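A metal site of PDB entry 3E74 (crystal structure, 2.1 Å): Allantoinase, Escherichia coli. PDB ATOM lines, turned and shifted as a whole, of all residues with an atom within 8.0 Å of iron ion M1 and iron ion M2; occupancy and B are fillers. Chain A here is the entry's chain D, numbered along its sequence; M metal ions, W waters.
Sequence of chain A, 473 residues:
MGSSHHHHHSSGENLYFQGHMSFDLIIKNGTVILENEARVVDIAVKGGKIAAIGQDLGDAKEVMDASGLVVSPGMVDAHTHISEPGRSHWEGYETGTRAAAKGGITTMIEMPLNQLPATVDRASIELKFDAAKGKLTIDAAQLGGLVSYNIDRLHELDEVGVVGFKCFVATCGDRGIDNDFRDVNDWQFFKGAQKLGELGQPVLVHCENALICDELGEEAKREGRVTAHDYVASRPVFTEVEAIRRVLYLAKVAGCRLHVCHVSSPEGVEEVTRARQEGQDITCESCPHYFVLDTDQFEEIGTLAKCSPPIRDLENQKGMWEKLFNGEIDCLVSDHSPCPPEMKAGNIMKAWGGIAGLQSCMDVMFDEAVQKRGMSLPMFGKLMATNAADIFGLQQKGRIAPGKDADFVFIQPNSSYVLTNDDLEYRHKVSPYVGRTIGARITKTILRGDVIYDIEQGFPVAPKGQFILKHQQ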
ATOM      1  N   HIS A  79      20.229 -10.796 -11.188  1.00  0.00           N
ATOM      2  CA  HIS A  79      21.447 -11.439 -10.714  1.00  0.00           C
ATOM      3  C   HIS A  79      21.554 -12.889 -11.201  1.00  0.00           C
ATOM      4  O   HIS A  79      21.349 -13.827 -10.434  1.00  0.00           O
ATOM      5  CB  HIS A  79      21.435 -11.405  -9.186  1.00  0.00           C
ATOM      6  CG  HIS A  79      22.784 -11.547  -8.566  1.00  0.00           C
ATOM      7  ND1 HIS A  79      23.241 -10.691  -7.593  1.00  0.00           N
ATOM      8  CD2 HIS A  79      23.775 -12.451  -8.769  1.00  0.00           C
ATOM      9  CE1 HIS A  79      24.446 -11.059  -7.211  1.00  0.00           C
ATOM     10  NE2 HIS A  79      24.798 -12.125  -7.917  1.00  0.00           N
ATOM     11  N   THR A  80      21.893 -13.050 -12.475  1.00  0.00           N
ATOM     12  CA  THR A  80      21.991 -14.384 -13.053  1.00  0.00           C
ATOM     13  C   THR A  80      23.378 -14.770 -13.515  1.00  0.00           C
ATOM     14  O   THR A  80      24.040 -14.020 -14.214  1.00  0.00           O
ATOM     15  CB  THR A  80      21.096 -14.546 -14.284  1.00  0.00           C
ATOM     16  OG1 THR A  80      19.829 -13.941 -14.041  1.00  0.00           O
ATOM     17  CG2 THR A  80      20.875 -16.023 -14.573  1.00  0.00           C
ATOM     18  N   HIS A  81      23.813 -15.968 -13.146  1.00  0.00           N
ATOM     19  CA  HIS A  81      25.095 -16.476 -13.593  1.00  0.00           C
ATOM     20  C   HIS A  81      24.768 -17.581 -14.583  1.00  0.00           C
ATOM     21  O   HIS A  81      23.956 -18.451 -14.305  1.00  0.00           O
ATOM     22  CB  HIS A  81      25.904 -17.032 -12.427  1.00  0.00           C
ATOM     23  CG  HIS A  81      26.443 -15.991 -11.492  1.00  0.00           C
ATOM     24  ND1 HIS A  81      27.559 -15.230 -11.783  1.00  0.00           N
ATOM     25  CD2 HIS A  81      25.999 -15.558 -10.285  1.00  0.00           C
ATOM     26  CE1 HIS A  81      27.789 -14.386 -10.799  1.00  0.00           C
ATOM     27  NE2 HIS A  81      26.850 -14.563  -9.872  1.00  0.00           N
ATOM     28  N   MET A 111      25.541 -11.737 -15.018  1.00  0.00           N
ATOM     29  CA  MET A 111      26.696 -11.345 -14.236  1.00  0.00           C
ATOM     30  C   MET A 111      27.894 -11.507 -15.165  1.00  0.00           C
ATOM     31  O   MET A 111      27.878 -12.365 -16.047  1.00  0.00           O
ATOM     32  CB  MET A 111      26.795 -12.227 -13.013  1.00  0.00           C
ATOM     33  CG  MET A 111      25.878 -11.774 -11.883  1.00  0.00           C
ATOM     34  SD  MET A 111      26.482 -10.067 -11.138  1.00  0.00           S
ATOM     35  CE  MET A 111      24.787  -9.276 -10.567  1.00  0.00           C
ATOM     36  N   LEU A 113      31.584 -11.896 -14.222  1.00  0.00           N
ATOM     37  CA  LEU A 113      32.610 -12.839 -13.856  1.00  0.00           C
ATOM     38  C   LEU A 113      31.991 -14.218 -13.661  1.00  0.00           C
ATOM     39  O   LEU A 113      30.795 -14.404 -13.925  1.00  0.00           O
ATOM     40  CB  LEU A 113      33.334 -12.362 -12.592  1.00  0.00           C
ATOM     41  CG  LEU A 113      33.709 -10.862 -12.599  1.00  0.00           C
ATOM     42  CD1 LEU A 113      34.575 -10.558 -11.374  1.00  0.00           C
ATOM     43  CD2 LEU A 113      34.447 -10.497 -13.861  1.00  0.00           C
ATOM     44  N   ASN A 114      32.803 -15.186 -13.237  1.00  0.00           N
ATOM     45  CA  ASN A 114      32.351 -16.563 -13.037  1.00  0.00           C
ATOM     46  C   ASN A 114      32.123 -17.199 -14.404  1.00  0.00           C
ATOM     47  O   ASN A 114      31.427 -18.207 -14.514  1.00  0.00           O
ATOM     48  CB  ASN A 114      31.027 -16.608 -12.251  1.00  0.00           C
ATOM     49  CG  ASN A 114      31.136 -15.982 -10.857  1.00  0.00           C
ATOM     50  OD1 ASN A 114      31.351 -14.775 -10.717  1.00  0.00           O
ATOM     51  ND2 ASN A 114      30.988 -16.822  -9.818  1.00  0.00           N
ATOM     52  N   KCX A 166      29.822  -5.070 -12.052  1.00  0.00           N
ATOM     53  CA  KCX A 166      29.913  -5.890 -10.843  1.00  0.00           C
ATOM     54  CB  KCX A 166      29.446  -7.309 -11.174  1.00  0.00           C
ATOM     55  CG  KCX A 166      28.688  -8.017 -10.081  1.00  0.00           C
ATOM     56  CD  KCX A 166      29.538  -8.548  -8.966  1.00  0.00           C
ATOM     57  CE  KCX A 166      28.652  -8.728  -7.725  1.00  0.00           C
ATOM     58  NZ  KCX A 166      28.755 -10.043  -7.076  1.00  0.00           N
ATOM     59  C   KCX A 166      31.359  -5.947 -10.345  1.00  0.00           C
ATOM     60  O   KCX A 166      32.285  -5.908 -11.144  1.00  0.00           O
ATOM     61  CX  KCX A 166      28.196 -11.167  -7.531  1.00  0.00           C
ATOM     62  OQ1 KCX A 166      28.339 -12.223  -6.890  1.00  0.00           O
ATOM     63  OQ2 KCX A 166      27.536 -11.111  -8.589  1.00  0.00           O
ATOM     64  N   CYS A 167      31.546  -6.078  -9.041  1.00  0.00           N
ATOM     65  CA  CYS A 167      32.888  -6.208  -8.481  1.00  0.00           C
ATOM     66  C   CYS A 167      32.800  -6.798  -7.089  1.00  0.00           C
ATOM     67  O   CYS A 167      31.717  -6.844  -6.489  1.00  0.00           O
ATOM     68  CB  CYS A 167      33.610  -4.853  -8.414  1.00  0.00           C
ATOM     69  SG  CYS A 167      33.003  -3.714  -7.126  1.00  0.00           S
ATOM     70  N   PHE A 168      33.935  -7.279  -6.602  1.00  0.00           N
ATOM     71  CA  PHE A 168      34.050  -7.850  -5.258  1.00  0.00           C
ATOM     72  C   PHE A 168      35.167  -7.074  -4.603  1.00  0.00           C
ATOM     73  O   PHE A 168      36.268  -6.985  -5.140  1.00  0.00           O
ATOM     74  CB  PHE A 168      34.428  -9.339  -5.318  1.00  0.00           C
ATOM     75  CG  PHE A 168      33.442 -10.184  -6.062  1.00  0.00           C
ATOM     76  CD1 PHE A 168      33.360 -10.140  -7.459  1.00  0.00           C
ATOM     77  CD2 PHE A 168      32.558 -11.022  -5.378  1.00  0.00           C
ATOM     78  CE1 PHE A 168      32.428 -10.912  -8.155  1.00  0.00           C
ATOM     79  CE2 PHE A 168      31.613 -11.801  -6.064  1.00  0.00           C
ATOM     80  CZ  PHE A 168      31.543 -11.742  -7.455  1.00  0.00           C
ATOM     81  N   VAL A 205      27.912  -4.465  -6.108  1.00  0.00           N
ATOM     82  CA  VAL A 205      28.963  -5.052  -5.277  1.00  0.00           C
ATOM     83  C   VAL A 205      28.553  -6.230  -4.420  1.00  0.00           C
ATOM     84  O   VAL A 205      27.478  -6.244  -3.818  1.00  0.00           O
ATOM     85  CB  VAL A 205      29.520  -3.975  -4.296  1.00  0.00           C
ATOM     86  CG1 VAL A 205      30.596  -4.596  -3.418  1.00  0.00           C
ATOM     87  CG2 VAL A 205      30.041  -2.745  -5.058  1.00  0.00           C
ATOM     88  N   HIS A 206      29.420  -7.245  -4.363  1.00  0.00           N
ATOM     89  CA  HIS A 206      29.210  -8.400  -3.484  1.00  0.00           C
ATOM     90  C   HIS A 206      29.834  -7.878  -2.171  1.00  0.00           C
ATOM     91  O   HIS A 206      31.015  -7.552  -2.129  1.00  0.00           O
ATOM     92  CB  HIS A 206      29.981  -9.634  -3.984  1.00  0.00           C
ATOM     93  CG  HIS A 206      29.998 -10.772  -3.012  1.00  0.00           C
ATOM     94  ND1 HIS A 206      29.384 -11.977  -3.262  1.00  0.00           N
ATOM     95  CD2 HIS A 206      30.562 -10.892  -1.778  1.00  0.00           C
ATOM     96  CE1 HIS A 206      29.554 -12.784  -2.228  1.00  0.00           C
ATOM     97  NE2 HIS A 206      30.270 -12.143  -1.311  1.00  0.00           N
ATOM     98  N   CYS A 207      29.042  -7.809  -1.109  1.00  0.00           N
ATOM     99  CA  CYS A 207      29.512  -7.256   0.156  1.00  0.00           C
ATOM    100  C   CYS A 207      29.750  -8.151   1.372  1.00  0.00           C
ATOM    101  O   CYS A 207      28.838  -8.359   2.178  1.00  0.00           O
ATOM    102  CB  CYS A 207      28.570  -6.131   0.588  1.00  0.00           C
ATOM    103  SG  CYS A 207      28.561  -4.674  -0.458  1.00  0.00           S
ATOM    104  N   GLU A 208      30.975  -8.632   1.507  1.00  0.00           N
ATOM    105  CA  GLU A 208      31.395  -9.448   2.661  1.00  0.00           C
ATOM    106  C   GLU A 208      32.882  -9.207   2.801  1.00  0.00           C
ATOM    107  O   GLU A 208      33.575  -8.988   1.802  1.00  0.00           O
ATOM    108  CB  GLU A 208      31.199 -10.952   2.435  1.00  0.00           C
ATOM    109  CG  GLU A 208      29.782 -11.470   2.376  1.00  0.00           C
ATOM    110  CD  GLU A 208      29.763 -12.990   2.257  1.00  0.00           C
ATOM    111  OE1 GLU A 208      30.150 -13.515   1.184  1.00  0.00           O
ATOM    112  OE2 GLU A 208      29.376 -13.678   3.230  1.00  0.00           O
ATOM    113  N   CYS A 261      24.385  -6.187  -3.667  1.00  0.00           N
ATOM    114  CA  CYS A 261      23.915  -7.507  -4.051  1.00  0.00           C
ATOM    115  C   CYS A 261      23.547  -8.393  -2.885  1.00  0.00           C
ATOM    116  O   CYS A 261      24.063  -8.226  -1.776  1.00  0.00           O
ATOM    117  CB  CYS A 261      24.967  -8.234  -4.908  1.00  0.00           C
ATOM    118  SG  CYS A 261      25.244  -7.529  -6.558  1.00  0.00           S
ATOM    119  N   HIS A 262      22.652  -9.339  -3.155  1.00  0.00           N
ATOM    120  CA  HIS A 262      22.182 -10.319  -2.172  1.00  0.00           C
ATOM    121  C   HIS A 262      22.447 -10.035  -0.697  1.00  0.00           C
ATOM    122  O   HIS A 262      23.384 -10.579  -0.117  1.00  0.00           O
ATOM    123  CB  HIS A 262      22.787 -11.677  -2.511  1.00  0.00           C
ATOM    124  CG  HIS A 262      24.255 -11.628  -2.794  1.00  0.00           C
ATOM    125  ND1 HIS A 262      25.157 -11.123  -1.894  1.00  0.00           N
ATOM    126  CD2 HIS A 262      24.962 -12.030  -3.875  1.00  0.00           C
ATOM    127  CE1 HIS A 262      26.375 -11.208  -2.410  1.00  0.00           C
ATOM    128  NE2 HIS A 262      26.286 -11.757  -3.614  1.00  0.00           N
ATOM    129  N   GLU A 285      19.176  -5.736  -3.014  1.00  0.00           N
ATOM    130  CA  GLU A 285      18.341  -6.852  -3.453  1.00  0.00           C
ATOM    131  C   GLU A 285      18.607  -8.012  -2.512  1.00  0.00           C
ATOM    132  O   GLU A 285      19.570  -7.997  -1.763  1.00  0.00           O
ATOM    133  CB  GLU A 285      18.768  -7.308  -4.858  1.00  0.00           C
ATOM    134  CG  GLU A 285      20.210  -7.849  -4.800  1.00  0.00           C
ATOM    135  CD  GLU A 285      20.805  -8.348  -6.109  1.00  0.00           C
ATOM    136  OE1 GLU A 285      20.446  -7.836  -7.193  1.00  0.00           O
ATOM    137  OE2 GLU A 285      21.665  -9.256  -6.045  1.00  0.00           O
ATOM    138  N   CYS A 287      17.473 -12.566  -2.158  1.00  0.00           N
ATOM    139  CA  CYS A 287      17.082 -13.715  -2.956  1.00  0.00           C
ATOM    140  C   CYS A 287      16.103 -14.630  -2.213  1.00  0.00           C
ATOM    141  O   CYS A 287      16.083 -14.661  -0.972  1.00  0.00           O
ATOM    142  CB  CYS A 287      18.316 -14.522  -3.333  1.00  0.00           C
ATOM    143  SG  CYS A 287      19.731 -13.537  -3.760  1.00  0.00           S
ATOM    144  N   TYR A 290      16.942 -16.530   1.111  1.00  0.00           N
ATOM    145  CA  TYR A 290      17.105 -15.795   2.368  1.00  0.00           C
ATOM    146  C   TYR A 290      15.732 -15.577   3.029  1.00  0.00           C
ATOM    147  O   TYR A 290      15.647 -15.144   4.198  1.00  0.00           O
ATOM    148  CB  TYR A 290      17.781 -14.438   2.109  1.00  0.00           C
ATOM    149  CG  TYR A 290      19.172 -14.571   1.541  1.00  0.00           C
ATOM    150  CD1 TYR A 290      20.148 -15.298   2.229  1.00  0.00           C
ATOM    151  CD2 TYR A 290      19.503 -14.013   0.315  1.00  0.00           C
ATOM    152  CE1 TYR A 290      21.420 -15.478   1.681  1.00  0.00           C
ATOM    153  CE2 TYR A 290      20.771 -14.177  -0.235  1.00  0.00           C
ATOM    154  CZ  TYR A 290      21.728 -14.915   0.451  1.00  0.00           C
ATOM    155  OH  TYR A 290      22.990 -15.077  -0.086  1.00  0.00           O
ATOM    156  N   CYS A 307      25.719 -21.195   0.227  1.00  0.00           N
ATOM    157  CA  CYS A 307      25.937 -20.045  -0.655  1.00  0.00           C
ATOM    158  C   CYS A 307      26.763 -18.964   0.059  1.00  0.00           C
ATOM    159  O   CYS A 307      26.831 -18.967   1.287  1.00  0.00           O
ATOM    160  CB  CYS A 307      24.596 -19.477  -1.132  1.00  0.00           C
ATOM    161  SG  CYS A 307      23.445 -19.150   0.202  1.00  0.00           S
ATOM    162  N   SER A 308      27.384 -18.079  -0.715  1.00  0.00           N
ATOM    163  CA  SER A 308      28.246 -17.018  -0.173  1.00  0.00           C
ATOM    164  C   SER A 308      27.553 -16.314   0.981  1.00  0.00           C
ATOM    165  O   SER A 308      27.694 -16.770   2.118  1.00  0.00           O
ATOM    166  CB  SER A 308      28.638 -16.011  -1.253  1.00  0.00           C
ATOM    167  OG  SER A 308      29.442 -16.634  -2.242  1.00  0.00           O
ATOM    168  N   PRO A 309      26.839 -15.194   0.735  1.00  0.00           N
ATOM    169  CA  PRO A 309      26.240 -14.699   1.987  1.00  0.00           C
ATOM    170  C   PRO A 309      25.436 -15.934   2.437  1.00  0.00           C
ATOM    171  O   PRO A 309      24.628 -16.455   1.681  1.00  0.00           O
ATOM    172  CB  PRO A 309      25.329 -13.546   1.510  1.00  0.00           C
ATOM    173  CG  PRO A 309      25.892 -13.161   0.198  1.00  0.00           C
ATOM    174  CD  PRO A 309      26.322 -14.472  -0.425  1.00  0.00           C
ATOM    175  N   SER A 334      17.617 -14.220  -8.305  1.00  0.00           N
ATOM    176  CA  SER A 334      17.975 -15.608  -8.046  1.00  0.00           C
ATOM    177  C   SER A 334      19.392 -15.838  -7.546  1.00  0.00           C
ATOM    178  O   SER A 334      19.603 -16.600  -6.621  1.00  0.00           O
ATOM    179  CB  SER A 334      17.807 -16.425  -9.319  1.00  0.00           C
ATOM    180  OG  SER A 334      18.798 -16.052 -10.252  1.00  0.00           O
ATOM    181  N   ASP A 335      20.348 -15.146  -8.155  1.00  0.00           N
ATOM    182  CA  ASP A 335      21.764 -15.344  -7.864  1.00  0.00           C
ATOM    183  C   ASP A 335      21.997 -16.825  -8.197  1.00  0.00           C
ATOM    184  O   ASP A 335      22.718 -17.551  -7.521  1.00  0.00           O
ATOM    185  CB  ASP A 335      22.128 -15.053  -6.402  1.00  0.00           C
ATOM    186  CG  ASP A 335      23.630 -15.164  -6.174  1.00  0.00           C
ATOM    187  OD1 ASP A 335      24.375 -15.127  -7.178  1.00  0.00           O
ATOM    188  OD2 ASP A 335      24.083 -15.267  -5.013  1.00  0.00           O
ATOM    189  N   HIS A 336      21.345 -17.266  -9.267  1.00  0.00           N
ATOM    190  CA  HIS A 336      21.474 -18.632  -9.707  1.00  0.00           C
ATOM    191  C   HIS A 336      22.949 -18.943  -9.937  1.00  0.00           C
ATOM    192  O   HIS A 336      23.615 -18.333 -10.770  1.00  0.00           O
ATOM    193  CB  HIS A 336      20.683 -18.828 -10.995  1.00  0.00           C
ATOM    194  CG  HIS A 336      20.733 -20.223 -11.515  1.00  0.00           C
ATOM    195  ND1 HIS A 336      20.217 -21.294 -10.813  1.00  0.00           N
ATOM    196  CD2 HIS A 336      21.219 -20.733 -12.665  1.00  0.00           C
ATOM    197  CE1 HIS A 336      20.382 -22.401 -11.518  1.00  0.00           C
ATOM    198  NE2 HIS A 336      20.987 -22.085 -12.646  1.00  0.00           N
ATOM    199  N   SER A 337      23.458 -19.912  -9.183  1.00  0.00           N
ATOM    200  CA  SER A 337      24.856 -20.323  -9.257  1.00  0.00           C
ATOM    201  C   SER A 337      24.948 -21.836  -9.335  1.00  0.00           C
ATOM    202  O   SER A 337      25.118 -22.508  -8.316  1.00  0.00           O
ATOM    203  CB  SER A 337      25.595 -19.823  -8.018  1.00  0.00           C
ATOM    204  OG  SER A 337      25.509 -18.406  -7.940  1.00  0.00           O
ATOM    205  N   GLY A 354      26.905 -21.939  -3.814  1.00  0.00           N
ATOM    206  CA  GLY A 354      26.019 -21.499  -4.887  1.00  0.00           C
ATOM    207  C   GLY A 354      24.672 -22.175  -4.830  1.00  0.00           C
ATOM    208  O   GLY A 354      24.558 -23.344  -4.466  1.00  0.00           O
HETATM  209 FE    FE M   1      26.533 -14.020  -7.595  1.00  0.00          FE
HETATM  210 FE    FE M   2      27.995 -12.903  -4.702  1.00  0.00          FE
HETATM  211  O   HOH W   1      29.333 -15.035  -6.537  1.00  0.00           O
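The side-chain carboxylate (OE1) of Glu 208 sits at hydrogen-bond distance from a ring nitrogen (NE2) of His 206.
O of Cys 167 sits at hydrogen-bond distance from N of His 206, at 3.2 Å.
The side-chain sulfur (SD) of Met 111 lies close to OQ2 of KCX 166.
The side-chain carboxylate (OE2) of Glu 285 is in hydrogen-bond range of the backbone NH (N) of His 262.
The backbone carbonyl oxygen (O) of His 336 sits close to the backbone NH (N) of His 81, at 3.4 Å.
The backbone carbonyl oxygen of Asp 335 is in hydrogen-bond range of the side-chain hydroxyl of Ser 337 (2.9 Å).
ND1 of His 79 is in hydrogen-bond range of OE2 of Glu 285.
OG of Ser 334 is in hydrogen-bond range of O of His 79 (3.4 Å).
Four residues have an atom within 4 Å of iron ion M1: His 79, His 81, KCX 166 and Asp 335.
Along chain A the residues within 4 Å of iron ion M1 span positions 79 to 335.
The nearest printed residue that does not touch iron ion M1 is His 262 (4.5 Å).
The nearest printed residue that does not touch iron ion M2 is Phe 168 (4.02 Å).
ND1 of His 206 binds iron ion M2.
OQ1 of KCX 166 binds iron ion M2 (2.3 Å).
NE2 of His 262 is bound to iron ion M2, 2.3 Å away.
Iron ion M1 is bound by a ring nitrogen (NE2) of His 81 (2.4 Å), the side-chain carboxylate (OD1) of Asp 335 (2.5 Å), a ring nitrogen (NE2) of His 79 (2.6 Å) and OQ1 of KCX 166 (2.6 Å).
Iron ion M1 has four donor atoms within binding distance.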
